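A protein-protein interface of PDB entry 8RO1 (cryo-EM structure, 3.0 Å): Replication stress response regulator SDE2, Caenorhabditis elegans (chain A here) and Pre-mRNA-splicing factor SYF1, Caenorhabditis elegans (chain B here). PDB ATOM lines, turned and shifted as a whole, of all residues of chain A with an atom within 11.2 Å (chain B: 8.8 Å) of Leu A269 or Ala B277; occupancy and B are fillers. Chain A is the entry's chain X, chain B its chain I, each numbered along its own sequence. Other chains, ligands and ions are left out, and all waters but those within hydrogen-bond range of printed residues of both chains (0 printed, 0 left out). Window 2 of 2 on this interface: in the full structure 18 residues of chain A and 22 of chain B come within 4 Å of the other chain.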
ATOM      1  N   GLU A 260      19.124 -19.653  23.096  1.00  0.00           N
ATOM      2  CA  GLU A 260      19.072 -19.851  24.539  1.00  0.00           C
ATOM      3  C   GLU A 260      20.421 -20.279  25.102  1.00  0.00           C
ATOM      4  O   GLU A 260      20.887 -19.707  26.092  1.00  0.00           O
ATOM      5  CB  GLU A 260      18.000 -20.883  24.889  1.00  0.00           C
ATOM      6  CG  GLU A 260      16.570 -20.413  24.664  1.00  0.00           C
ATOM      7  CD  GLU A 260      15.948 -19.804  25.909  1.00  0.00           C
ATOM      8  OE1 GLU A 260      16.608 -18.977  26.568  1.00  0.00           O
ATOM      9  OE2 GLU A 260      14.794 -20.154  26.230  1.00  0.00           O
ATOM     10  N   ASP A 261      21.061 -21.288  24.503  1.00  0.00           N
ATOM     11  CA  ASP A 261      22.432 -21.606  24.903  1.00  0.00           C
ATOM     12  C   ASP A 261      23.367 -20.425  24.655  1.00  0.00           C
ATOM     13  O   ASP A 261      24.329 -20.227  25.408  1.00  0.00           O
ATOM     14  CB  ASP A 261      22.934 -22.876  24.208  1.00  0.00           C
ATOM     15  CG  ASP A 261      23.446 -22.626  22.815  1.00  0.00           C
ATOM     16  OD1 ASP A 261      22.621 -22.348  21.934  1.00  0.00           O
ATOM     17  OD2 ASP A 261      24.674 -22.689  22.605  1.00  0.00           O
ATOM     18  N   ALA A 262      23.135 -19.668  23.574  1.00  0.00           N
ATOM     19  CA  ALA A 262      23.943 -18.482  23.296  1.00  0.00           C
ATOM     20  C   ALA A 262      23.921 -17.526  24.480  1.00  0.00           C
ATOM     21  O   ALA A 262      24.947 -16.936  24.832  1.00  0.00           O
ATOM     22  CB  ALA A 262      23.448 -17.779  22.039  1.00  0.00           C
ATOM     23  N   CYS A 263      22.757 -17.364  25.109  1.00  0.00           N
ATOM     24  CA  CYS A 263      22.710 -16.607  26.352  1.00  0.00           C
ATOM     25  C   CYS A 263      23.522 -17.300  27.435  1.00  0.00           C
ATOM     26  O   CYS A 263      24.251 -16.644  28.186  1.00  0.00           O
ATOM     27  CB  CYS A 263      21.267 -16.427  26.826  1.00  0.00           C
ATOM     28  SG  CYS A 263      20.180 -15.424  25.802  1.00  0.00           S
ATOM     29  N   GLU A 264      23.436 -18.628  27.506  1.00  0.00           N
ATOM     30  CA  GLU A 264      24.133 -19.360  28.558  1.00  0.00           C
ATOM     31  C   GLU A 264      25.640 -19.217  28.394  1.00  0.00           C
ATOM     32  O   GLU A 264      26.348 -18.875  29.348  1.00  0.00           O
ATOM     33  CB  GLU A 264      23.698 -20.828  28.545  1.00  0.00           C
ATOM     34  CG  GLU A 264      24.359 -21.723  29.589  1.00  0.00           C
ATOM     35  CD  GLU A 264      23.884 -23.162  29.498  1.00  0.00           C
ATOM     36  OE1 GLU A 264      22.757 -23.390  29.007  1.00  0.00           O
ATOM     37  OE2 GLU A 264      24.632 -24.064  29.927  1.00  0.00           O
ATOM     38  N   ALA A 265      26.150 -19.501  27.195  1.00  0.00           N
ATOM     39  CA  ALA A 265      27.562 -19.263  26.915  1.00  0.00           C
ATOM     40  C   ALA A 265      27.917 -17.789  27.075  1.00  0.00           C
ATOM     41  O   ALA A 265      29.005 -17.454  27.558  1.00  0.00           O
ATOM     42  CB  ALA A 265      27.905 -19.745  25.508  1.00  0.00           C
ATOM     43  N   GLY A 266      27.021 -16.892  26.667  1.00  0.00           N
ATOM     44  CA  GLY A 266      27.314 -15.473  26.779  1.00  0.00           C
ATOM     45  C   GLY A 266      27.357 -14.977  28.213  1.00  0.00           C
ATOM     46  O   GLY A 266      28.296 -14.283  28.610  1.00  0.00           O
ATOM     47  N   PHE A 267      26.356 -15.344  29.017  1.00  0.00           N
ATOM     48  CA  PHE A 267      26.278 -14.828  30.382  1.00  0.00           C
ATOM     49  C   PHE A 267      27.267 -15.501  31.315  1.00  0.00           C
ATOM     50  O   PHE A 267      27.704 -14.878  32.290  1.00  0.00           O
ATOM     51  CB  PHE A 267      24.854 -14.963  30.934  1.00  0.00           C
ATOM     52  CG  PHE A 267      23.847 -14.052  30.276  1.00  0.00           C
ATOM     53  CD1 PHE A 267      24.029 -12.679  30.277  1.00  0.00           C
ATOM     54  CD2 PHE A 267      22.713 -14.555  29.678  1.00  0.00           C
ATOM     55  CE1 PHE A 267      23.111 -11.842  29.686  1.00  0.00           C
ATOM     56  CE2 PHE A 267      21.797 -13.711  29.081  1.00  0.00           C
ATOM     57  CZ  PHE A 267      22.007 -12.360  29.071  1.00  0.00           C
ATOM     58  N   ALA A 268      27.627 -16.755  31.055  1.00  0.00           N
ATOM     59  CA  ALA A 268      28.731 -17.355  31.793  1.00  0.00           C
ATOM     60  C   ALA A 268      30.018 -16.568  31.582  1.00  0.00           C
ATOM     61  O   ALA A 268      30.743 -16.283  32.541  1.00  0.00           O
ATOM     62  CB  ALA A 268      28.913 -18.809  31.367  1.00  0.00           C
ATOM     63  N   LEU A 269      30.290 -16.165  30.342  1.00  0.00           N
ATOM     64  CA  LEU A 269      31.456 -15.333  30.060  1.00  0.00           C
ATOM     65  C   LEU A 269      31.324 -13.948  30.678  1.00  0.00           C
ATOM     66  O   LEU A 269      32.315 -13.383  31.155  1.00  0.00           O
ATOM     67  CB  LEU A 269      31.667 -15.234  28.551  1.00  0.00           C
ATOM     68  CG  LEU A 269      32.824 -14.363  28.054  1.00  0.00           C
ATOM     69  CD1 LEU A 269      33.471 -15.016  26.854  1.00  0.00           C
ATOM     70  CD2 LEU A 269      32.377 -12.962  27.675  1.00  0.00           C
ATOM     71  N   MET A 270      30.122 -13.370  30.641  1.00  0.00           N
ATOM     72  CA  MET A 270      29.901 -12.055  31.239  1.00  0.00           C
ATOM     73  C   MET A 270      30.238 -12.053  32.722  1.00  0.00           C
ATOM     74  O   MET A 270      30.830 -11.092  33.228  1.00  0.00           O
ATOM     75  CB  MET A 270      28.449 -11.620  31.023  1.00  0.00           C
ATOM     76  CG  MET A 270      28.078 -10.249  31.597  1.00  0.00           C
ATOM     77  SD  MET A 270      29.002  -8.892  30.856  1.00  0.00           S
ATOM     78  CE  MET A 270      28.301  -7.497  31.729  1.00  0.00           C
ATOM     79  N   LEU A 271      29.878 -13.117  33.433  1.00  0.00           N
ATOM     80  CA  LEU A 271      30.205 -13.193  34.851  1.00  0.00           C
ATOM     81  C   LEU A 271      31.710 -13.253  35.074  1.00  0.00           C
ATOM     82  O   LEU A 271      32.229 -12.616  35.998  1.00  0.00           O
ATOM     83  CB  LEU A 271      29.522 -14.409  35.471  1.00  0.00           C
ATOM     84  CG  LEU A 271      28.002 -14.309  35.609  1.00  0.00           C
ATOM     85  CD1 LEU A 271      27.410 -15.681  35.874  1.00  0.00           C
ATOM     86  CD2 LEU A 271      27.591 -13.331  36.705  1.00  0.00           C
ATOM     87  N   GLU A 272      32.427 -14.015  34.243  1.00  0.00           N
ATOM     88  CA  GLU A 272      33.884 -14.041  34.330  1.00  0.00           C
ATOM     89  C   GLU A 272      34.482 -12.660  34.093  1.00  0.00           C
ATOM     90  O   GLU A 272      35.405 -12.246  34.802  1.00  0.00           O
ATOM     91  CB  GLU A 272      34.456 -15.030  33.309  1.00  0.00           C
ATOM     92  CG  GLU A 272      33.975 -16.486  33.415  1.00  0.00           C
ATOM     93  CD  GLU A 272      33.619 -16.927  34.821  1.00  0.00           C
ATOM     94  OE1 GLU A 272      34.501 -16.884  35.700  1.00  0.00           O
ATOM     95  OE2 GLU A 272      32.450 -17.305  35.045  1.00  0.00           O
ATOM     96  N   MET A 273      33.960 -11.928  33.110  1.00  0.00           N
ATOM     97  CA  MET A 273      34.426 -10.565  32.877  1.00  0.00           C
ATOM     98  C   MET A 273      34.103  -9.647  34.049  1.00  0.00           C
ATOM     99  O   MET A 273      34.929  -8.817  34.441  1.00  0.00           O
ATOM    100  CB  MET A 273      33.809 -10.015  31.592  1.00  0.00           C
ATOM    101  CG  MET A 273      34.361 -10.639  30.326  1.00  0.00           C
ATOM    102  SD  MET A 273      33.614  -9.984  28.822  1.00  0.00           S
ATOM    103  CE  MET A 273      34.221  -8.299  28.821  1.00  0.00           C
ATOM    104  N   LYS A 274      32.906  -9.779  34.621  1.00  0.00           N
ATOM    105  CA  LYS A 274      32.529  -8.911  35.730  1.00  0.00           C
ATOM    106  C   LYS A 274      33.351  -9.174  36.986  1.00  0.00           C
ATOM    107  O   LYS A 274      33.532  -8.261  37.799  1.00  0.00           O
ATOM    108  CB  LYS A 274      31.043  -9.076  36.039  1.00  0.00           C
ATOM    109  CG  LYS A 274      30.461  -7.947  36.888  1.00  0.00           C
ATOM    110  CD  LYS A 274      28.936  -7.870  36.822  1.00  0.00           C
ATOM    111  CE  LYS A 274      28.254  -9.033  37.541  1.00  0.00           C
ATOM    112  NZ  LYS A 274      28.057  -8.740  38.986  1.00  0.00           N
ATOM    113  N   ARG A 275      33.871 -10.390  37.158  1.00  0.00           N
ATOM    114  CA  ARG A 275      34.741 -10.664  38.300  1.00  0.00           C
ATOM    115  C   ARG A 275      36.171 -10.197  38.056  1.00  0.00           C
ATOM    116  O   ARG A 275      36.797  -9.626  38.954  1.00  0.00           O
ATOM    117  CB  ARG A 275      34.733 -12.152  38.639  1.00  0.00           C
ATOM    118  CG  ARG A 275      33.421 -12.646  39.215  1.00  0.00           C
ATOM    119  CD  ARG A 275      33.567 -14.022  39.848  1.00  0.00           C
ATOM    120  NE  ARG A 275      34.097 -15.027  38.927  1.00  0.00           N
ATOM    121  CZ  ARG A 275      35.377 -15.351  38.775  1.00  0.00           C
ATOM    122  NH1 ARG A 275      35.715 -16.216  37.824  1.00  0.00           N
ATOM    123  NH2 ARG A 275      36.325 -14.878  39.572  1.00  0.00           N
ATOM    124  N   ASN A 276      36.706 -10.445  36.858  1.00  0.00           N
ATOM    125  CA  ASN A 276      38.074 -10.033  36.553  1.00  0.00           C
ATOM    126  C   ASN A 276      38.247  -8.522  36.632  1.00  0.00           C
ATOM    127  O   ASN A 276      39.348  -8.043  36.928  1.00  0.00           O
ATOM    128  CB  ASN A 276      38.481 -10.547  35.173  1.00  0.00           C
ATOM    129  CG  ASN A 276      38.667 -12.048  35.148  1.00  0.00           C
ATOM    130  OD1 ASN A 276      38.330 -12.740  36.109  1.00  0.00           O
ATOM    131  ND2 ASN A 276      39.215 -12.560  34.053  1.00  0.00           N
ATOM    132  N   SER A 277      37.191  -7.754  36.351  1.00  0.00           N
ATOM    133  CA  SER A 277      37.270  -6.306  36.526  1.00  0.00           C
ATOM    134  C   SER A 277      37.550  -5.927  37.976  1.00  0.00           C
ATOM    135  O   SER A 277      38.152  -4.878  38.235  1.00  0.00           O
ATOM    136  CB  SER A 277      35.973  -5.644  36.058  1.00  0.00           C
ATOM    137  OG  SER A 277      34.918  -5.889  36.974  1.00  0.00           O
ATOM    138  N   PRO B 239      33.176 -15.774  18.234  1.00  0.00           N
ATOM    139  CA  PRO B 239      33.435 -14.328  18.155  1.00  0.00           C
ATOM    140  C   PRO B 239      34.818 -13.941  18.634  1.00  0.00           C
ATOM    141  O   PRO B 239      35.471 -13.082  18.033  1.00  0.00           O
ATOM    142  CB  PRO B 239      32.367 -13.728  19.075  1.00  0.00           C
ATOM    143  CG  PRO B 239      31.391 -14.776  19.284  1.00  0.00           C
ATOM    144  CD  PRO B 239      32.133 -16.051  19.229  1.00  0.00           C
ATOM    145  N   VAL B 240      35.287 -14.584  19.705  1.00  0.00           N
ATOM    146  CA  VAL B 240      36.540 -14.180  20.330  1.00  0.00           C
ATOM    147  C   VAL B 240      37.732 -14.624  19.498  1.00  0.00           C
ATOM    148  O   VAL B 240      38.763 -13.942  19.471  1.00  0.00           O
ATOM    149  CB  VAL B 240      36.625 -14.750  21.764  1.00  0.00           C
ATOM    150  CG1 VAL B 240      37.928 -14.329  22.463  1.00  0.00           C
ATOM    151  CG2 VAL B 240      35.418 -14.339  22.607  1.00  0.00           C
ATOM    152  N   ALA B 270      22.725 -11.631  15.789  1.00  0.00           N
ATOM    153  CA  ALA B 270      22.606 -11.328  17.212  1.00  0.00           C
ATOM    154  C   ALA B 270      23.309 -12.372  18.067  1.00  0.00           C
ATOM    155  O   ALA B 270      23.934 -12.035  19.077  1.00  0.00           O
ATOM    156  CB  ALA B 270      21.138 -11.224  17.608  1.00  0.00           C
ATOM    157  N   ASP B 271      23.185 -13.646  17.693  1.00  0.00           N
ATOM    158  CA  ASP B 271      23.882 -14.735  18.374  1.00  0.00           C
ATOM    159  C   ASP B 271      25.385 -14.489  18.459  1.00  0.00           C
ATOM    160  O   ASP B 271      26.006 -14.746  19.494  1.00  0.00           O
ATOM    161  CB  ASP B 271      23.584 -16.046  17.641  1.00  0.00           C
ATOM    162  CG  ASP B 271      24.264 -17.267  18.265  1.00  0.00           C
ATOM    163  OD1 ASP B 271      24.832 -17.179  19.375  1.00  0.00           O
ATOM    164  OD2 ASP B 271      24.234 -18.337  17.619  1.00  0.00           O
ATOM    165  N   TYR B 272      25.986 -14.006  17.373  1.00  0.00           N
ATOM    166  CA  TYR B 272      27.395 -13.619  17.386  1.00  0.00           C
ATOM    167  C   TYR B 272      27.692 -12.574  18.452  1.00  0.00           C
ATOM    168  O   TYR B 272      28.647 -12.712  19.219  1.00  0.00           O
ATOM    169  CB  TYR B 272      27.784 -13.106  16.006  1.00  0.00           C
ATOM    170  CG  TYR B 272      29.037 -12.290  15.959  1.00  0.00           C
ATOM    171  CD1 TYR B 272      30.269 -12.891  15.987  1.00  0.00           C
ATOM    172  CD2 TYR B 272      28.990 -10.924  15.825  1.00  0.00           C
ATOM    173  CE1 TYR B 272      31.419 -12.158  15.920  1.00  0.00           C
ATOM    174  CE2 TYR B 272      30.142 -10.181  15.753  1.00  0.00           C
ATOM    175  CZ  TYR B 272      31.351 -10.803  15.804  1.00  0.00           C
ATOM    176  OH  TYR B 272      32.508 -10.069  15.732  1.00  0.00           O
ATOM    177  N   TYR B 273      26.894 -11.516  18.510  1.00  0.00           N
ATOM    178  CA  TYR B 273      27.118 -10.477  19.513  1.00  0.00           C
ATOM    179  C   TYR B 273      26.836 -10.962  20.927  1.00  0.00           C
ATOM    180  O   TYR B 273      27.541 -10.574  21.862  1.00  0.00           O
ATOM    181  CB  TYR B 273      26.305  -9.234  19.172  1.00  0.00           C
ATOM    182  CG  TYR B 273      26.883  -8.467  18.011  1.00  0.00           C
ATOM    183  CD1 TYR B 273      28.135  -7.895  18.094  1.00  0.00           C
ATOM    184  CD2 TYR B 273      26.199  -8.338  16.829  1.00  0.00           C
ATOM    185  CE1 TYR B 273      28.669  -7.213  17.058  1.00  0.00           C
ATOM    186  CE2 TYR B 273      26.737  -7.648  15.781  1.00  0.00           C
ATOM    187  CZ  TYR B 273      27.972  -7.091  15.902  1.00  0.00           C
ATOM    188  OH  TYR B 273      28.520  -6.393  14.861  1.00  0.00           O
ATOM    189  N   ILE B 274      25.823 -11.803  21.114  1.00  0.00           N
ATOM    190  CA  ILE B 274      25.535 -12.339  22.444  1.00  0.00           C
ATOM    191  C   ILE B 274      26.711 -13.177  22.938  1.00  0.00           C
ATOM    192  O   ILE B 274      27.124 -13.069  24.096  1.00  0.00           O
ATOM    193  CB  ILE B 274      24.217 -13.139  22.432  1.00  0.00           C
ATOM    194  CG1 ILE B 274      23.032 -12.203  22.179  1.00  0.00           C
ATOM    195  CG2 ILE B 274      23.972 -13.847  23.778  1.00  0.00           C
ATOM    196  CD1 ILE B 274      21.756 -12.898  21.724  1.00  0.00           C
ATOM    197  N   ARG B 275      27.267 -14.023  22.073  1.00  0.00           N
ATOM    198  CA  ARG B 275      28.453 -14.786  22.456  1.00  0.00           C
ATOM    199  C   ARG B 275      29.671 -13.902  22.684  1.00  0.00           C
ATOM    200  O   ARG B 275      30.545 -14.266  23.476  1.00  0.00           O
ATOM    201  CB  ARG B 275      28.772 -15.838  21.405  1.00  0.00           C
ATOM    202  CG  ARG B 275      27.774 -16.946  21.371  1.00  0.00           C
ATOM    203  CD  ARG B 275      28.182 -18.013  20.401  1.00  0.00           C
ATOM    204  NE  ARG B 275      27.047 -18.871  20.082  1.00  0.00           N
ATOM    205  CZ  ARG B 275      26.735 -20.005  20.702  1.00  0.00           C
ATOM    206  NH1 ARG B 275      25.627 -20.647  20.350  1.00  0.00           N
ATOM    207  NH2 ARG B 275      27.506 -20.529  21.645  1.00  0.00           N
ATOM    208  N   SER B 276      29.752 -12.747  22.034  1.00  0.00           N
ATOM    209  CA  SER B 276      30.791 -11.784  22.380  1.00  0.00           C
ATOM    210  C   SER B 276      30.492 -11.036  23.674  1.00  0.00           C
ATOM    211  O   SER B 276      31.334 -10.252  24.116  1.00  0.00           O
ATOM    212  CB  SER B 276      30.992 -10.778  21.246  1.00  0.00           C
ATOM    213  OG  SER B 276      32.247 -10.128  21.363  1.00  0.00           O
ATOM    214  N   ALA B 277      29.320 -11.254  24.278  1.00  0.00           N
ATOM    215  CA  ALA B 277      28.817 -10.497  25.426  1.00  0.00           C
ATOM    216  C   ALA B 277      28.690  -8.997  25.148  1.00  0.00           C
ATOM    217  O   ALA B 277      28.767  -8.183  26.069  1.00  0.00           O
ATOM    218  CB  ALA B 277      29.692 -10.734  26.659  1.00  0.00           C
ATOM    219  N   GLU B 278      28.500  -8.623  23.884  1.00  0.00           N
ATOM    220  CA  GLU B 278      28.257  -7.233  23.485  1.00  0.00           C
ATOM    221  C   GLU B 278      26.752  -6.960  23.411  1.00  0.00           C
ATOM    222  O   GLU B 278      26.202  -6.646  22.357  1.00  0.00           O
ATOM    223  CB  GLU B 278      28.960  -6.906  22.176  1.00  0.00           C
ATOM    224  CG  GLU B 278      30.474  -7.001  22.259  1.00  0.00           C
ATOM    225  CD  GLU B 278      31.154  -6.685  20.941  1.00  0.00           C
ATOM    226  OE1 GLU B 278      30.890  -5.597  20.385  1.00  0.00           O
ATOM    227  OE2 GLU B 278      31.955  -7.515  20.463  1.00  0.00           O
ATOM    228  N   PHE B 279      26.084  -7.106  24.558  1.00  0.00           N
ATOM    229  CA  PHE B 279      24.621  -7.093  24.610  1.00  0.00           C
ATOM    230  C   PHE B 279      24.015  -5.792  24.101  1.00  0.00           C
ATOM    231  O   PHE B 279      22.884  -5.798  23.608  1.00  0.00           O
ATOM    232  CB  PHE B 279      24.133  -7.349  26.032  1.00  0.00           C
ATOM    233  CG  PHE B 279      24.639  -8.615  26.622  1.00  0.00           C
ATOM    234  CD1 PHE B 279      24.330  -9.822  26.050  1.00  0.00           C
ATOM    235  CD2 PHE B 279      25.450  -8.596  27.731  1.00  0.00           C
ATOM    236  CE1 PHE B 279      24.797 -10.990  26.583  1.00  0.00           C
ATOM    237  CE2 PHE B 279      25.924  -9.760  28.271  1.00  0.00           C
ATOM    238  CZ  PHE B 279      25.609 -10.961  27.687  1.00  0.00           C
ATOM    239  N   GLU B 280      24.729  -4.675  24.206  1.00  0.00           N
ATOM    240  CA  GLU B 280      24.226  -3.434  23.625  1.00  0.00           C
ATOM    241  C   GLU B 280      24.085  -3.547  22.113  1.00  0.00           C
ATOM    242  O   GLU B 280      23.035  -3.209  21.555  1.00  0.00           O
ATOM    243  CB  GLU B 280      25.161  -2.277  23.983  1.00  0.00           C
ATOM    244  CG  GLU B 280      25.244  -1.936  25.472  1.00  0.00           C
ATOM    245  CD  GLU B 280      23.894  -1.687  26.123  1.00  0.00           C
ATOM    246  OE1 GLU B 280      23.011  -1.105  25.459  1.00  0.00           O
ATOM    247  OE2 GLU B 280      23.718  -2.080  27.294  1.00  0.00           O
ATOM    248  N   ARG B 281      25.114  -4.039  21.428  1.00  0.00           N
ATOM    249  CA  ARG B 281      24.990  -4.217  19.985  1.00  0.00           C
ATOM    250  C   ARG B 281      24.069  -5.377  19.638  1.00  0.00           C
ATOM    251  O   ARG B 281      23.533  -5.421  18.527  1.00  0.00           O
ATOM    252  CB  ARG B 281      26.363  -4.398  19.349  1.00  0.00           C
ATOM    253  CG  ARG B 281      27.201  -3.168  19.536  1.00  0.00           C
ATOM    254  CD  ARG B 281      28.206  -2.901  18.450  1.00  0.00           C
ATOM    255  NE  ARG B 281      29.369  -3.771  18.528  1.00  0.00           N
ATOM    256  CZ  ARG B 281      30.450  -3.657  17.768  1.00  0.00           C
ATOM    257  NH1 ARG B 281      31.456  -4.507  17.945  1.00  0.00           N
ATOM    258  NH2 ARG B 281      30.551  -2.724  16.831  1.00  0.00           N
ATOM    259  N   ALA B 282      23.904  -6.342  20.543  1.00  0.00           N
ATOM    260  CA  ALA B 282      22.898  -7.381  20.344  1.00  0.00           C
ATOM    261  C   ALA B 282      21.499  -6.791  20.276  1.00  0.00           C
ATOM    262  O   ALA B 282      20.682  -7.202  19.447  1.00  0.00           O
ATOM    263  CB  ALA B 282      22.973  -8.409  21.464  1.00  0.00           C
ATOM    264  N   PHE B 309      15.639 -13.794  24.283  1.00  0.00           N
ATOM    265  CA  PHE B 309      16.901 -13.208  24.721  1.00  0.00           C
ATOM    266  C   PHE B 309      16.721 -12.297  25.924  1.00  0.00           C
ATOM    267  O   PHE B 309      17.463 -12.396  26.904  1.00  0.00           O
ATOM    268  CB  PHE B 309      17.541 -12.420  23.588  1.00  0.00           C
ATOM    269  CG  PHE B 309      18.633 -11.524  24.044  1.00  0.00           C
ATOM    270  CD1 PHE B 309      19.792 -12.045  24.542  1.00  0.00           C
ATOM    271  CD2 PHE B 309      18.486 -10.162  24.001  1.00  0.00           C
ATOM    272  CE1 PHE B 309      20.793 -11.230  24.973  1.00  0.00           C
ATOM    273  CE2 PHE B 309      19.484  -9.339  24.428  1.00  0.00           C
ATOM    274  CZ  PHE B 309      20.640  -9.871  24.921  1.00  0.00           C
ATOM    275  N   GLU B 313      18.338 -12.681  30.083  1.00  0.00           N
ATOM    276  CA  GLU B 313      19.072 -11.594  30.720  1.00  0.00           C
ATOM    277  C   GLU B 313      18.394 -11.177  32.018  1.00  0.00           C
ATOM    278  O   GLU B 313      19.053 -11.007  33.049  1.00  0.00           O
ATOM    279  CB  GLU B 313      19.211 -10.407  29.774  1.00  0.00           C
ATOM    280  CG  GLU B 313      20.280  -9.428  30.215  1.00  0.00           C
ATOM    281  CD  GLU B 313      20.497  -8.303  29.228  1.00  0.00           C
ATOM    282  OE1 GLU B 313      19.767  -8.243  28.217  1.00  0.00           O
ATOM    283  OE2 GLU B 313      21.388  -7.463  29.469  1.00  0.00           O
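Of the 18 printed residues of chain A, 8 touch a printed residue of chain B. Printed residues of chain A that touch a printed residue of chain B: Asp A261, Ala A262, Cys A263, Ala A265, Gly A266, Phe A267, Leu A269 and Met A270. Hydrophobic or aromatic side chains of chain A within 4 Å of the printed part of chain B: Ala A262, Ala A265, Phe A267, Leu A269 and Met A270. Along chain A the printed residues that touch a printed residue of chain B span positions 261 to 270. Printed residues of chain B that touch a printed residue of chain A: Asp B271, Ile B274, Arg B275, Ala B277, Phe B279, Phe B309 and Glu B313. Hydrophobic or aromatic side chains of chain B that line the printed part of chain A: Ile B274, Ala B277, Phe B279 and Phe B309. Among the printed residues, 12 pairs touch across the chains.
Among the printed residues, pairs that only touch across the chains: Ala A262 with Asp B271 (3.1 Å), Ala A262 with Ile B274 (3.4 Å), Ala A262 with Arg B275 (3.98 Å), Cys A263 with Ile B274 (3.95 Å), Cys A263 with Phe B309 (3.6 Å), Ala A265 with Arg B275 (3.96 Å), Gly A266 with Ile B274 (3.6 Å), Phe A267 with Phe B279 (3.3 Å), Phe A267 with Glu B313 (3.5 Å), Leu A269 with Ala B277 (3.6 Å) and Met A270 with Phe B279 (3.99 Å).
NE of Arg B275 lies within salt-bridge range of OD1 of Asp B271.
Of the printed residues of chain B, Ala A265 touches Arg B275 (3.96 Å). Of the printed residues of chain B, Phe A267 touches Phe B279 (3.3 Å) and Glu B313 (3.5 Å). No residue of chain B comes within 4 Å of Ala A268. Of chain B, only Ala B277 comes within 4 Å of Leu A269. Printed residues of chain B within 4 Å of Met A270: Phe B279 (3.99 Å). Glu A272 touches none of the printed residues of chain B. Arg A275 touches none of the printed residues of chain B. Printed residues of chain A within 4 Å of Asp B271: Ala A262. Printed residues of chain A within 4 Å of Arg B275: Asp A261 (3.2 Å), Ala A262 (3.98 Å) and Ala A265 (3.96 Å). No residue of chain A comes within 4 Å of Ser B276. Ala B277 touches just one residue of chain A: Leu A269 (3.6 Å). No residue of chain A comes within 4 Å of Glu B278. The nearest residue of chain B that does not touch Leu A269 is Arg B275 (4.5 Å).
The guanidinium group (NH1) of Arg B275 is in salt-bridge range of the side-chain carboxylate (OD2) of Asp A261, 3.2 Å away.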
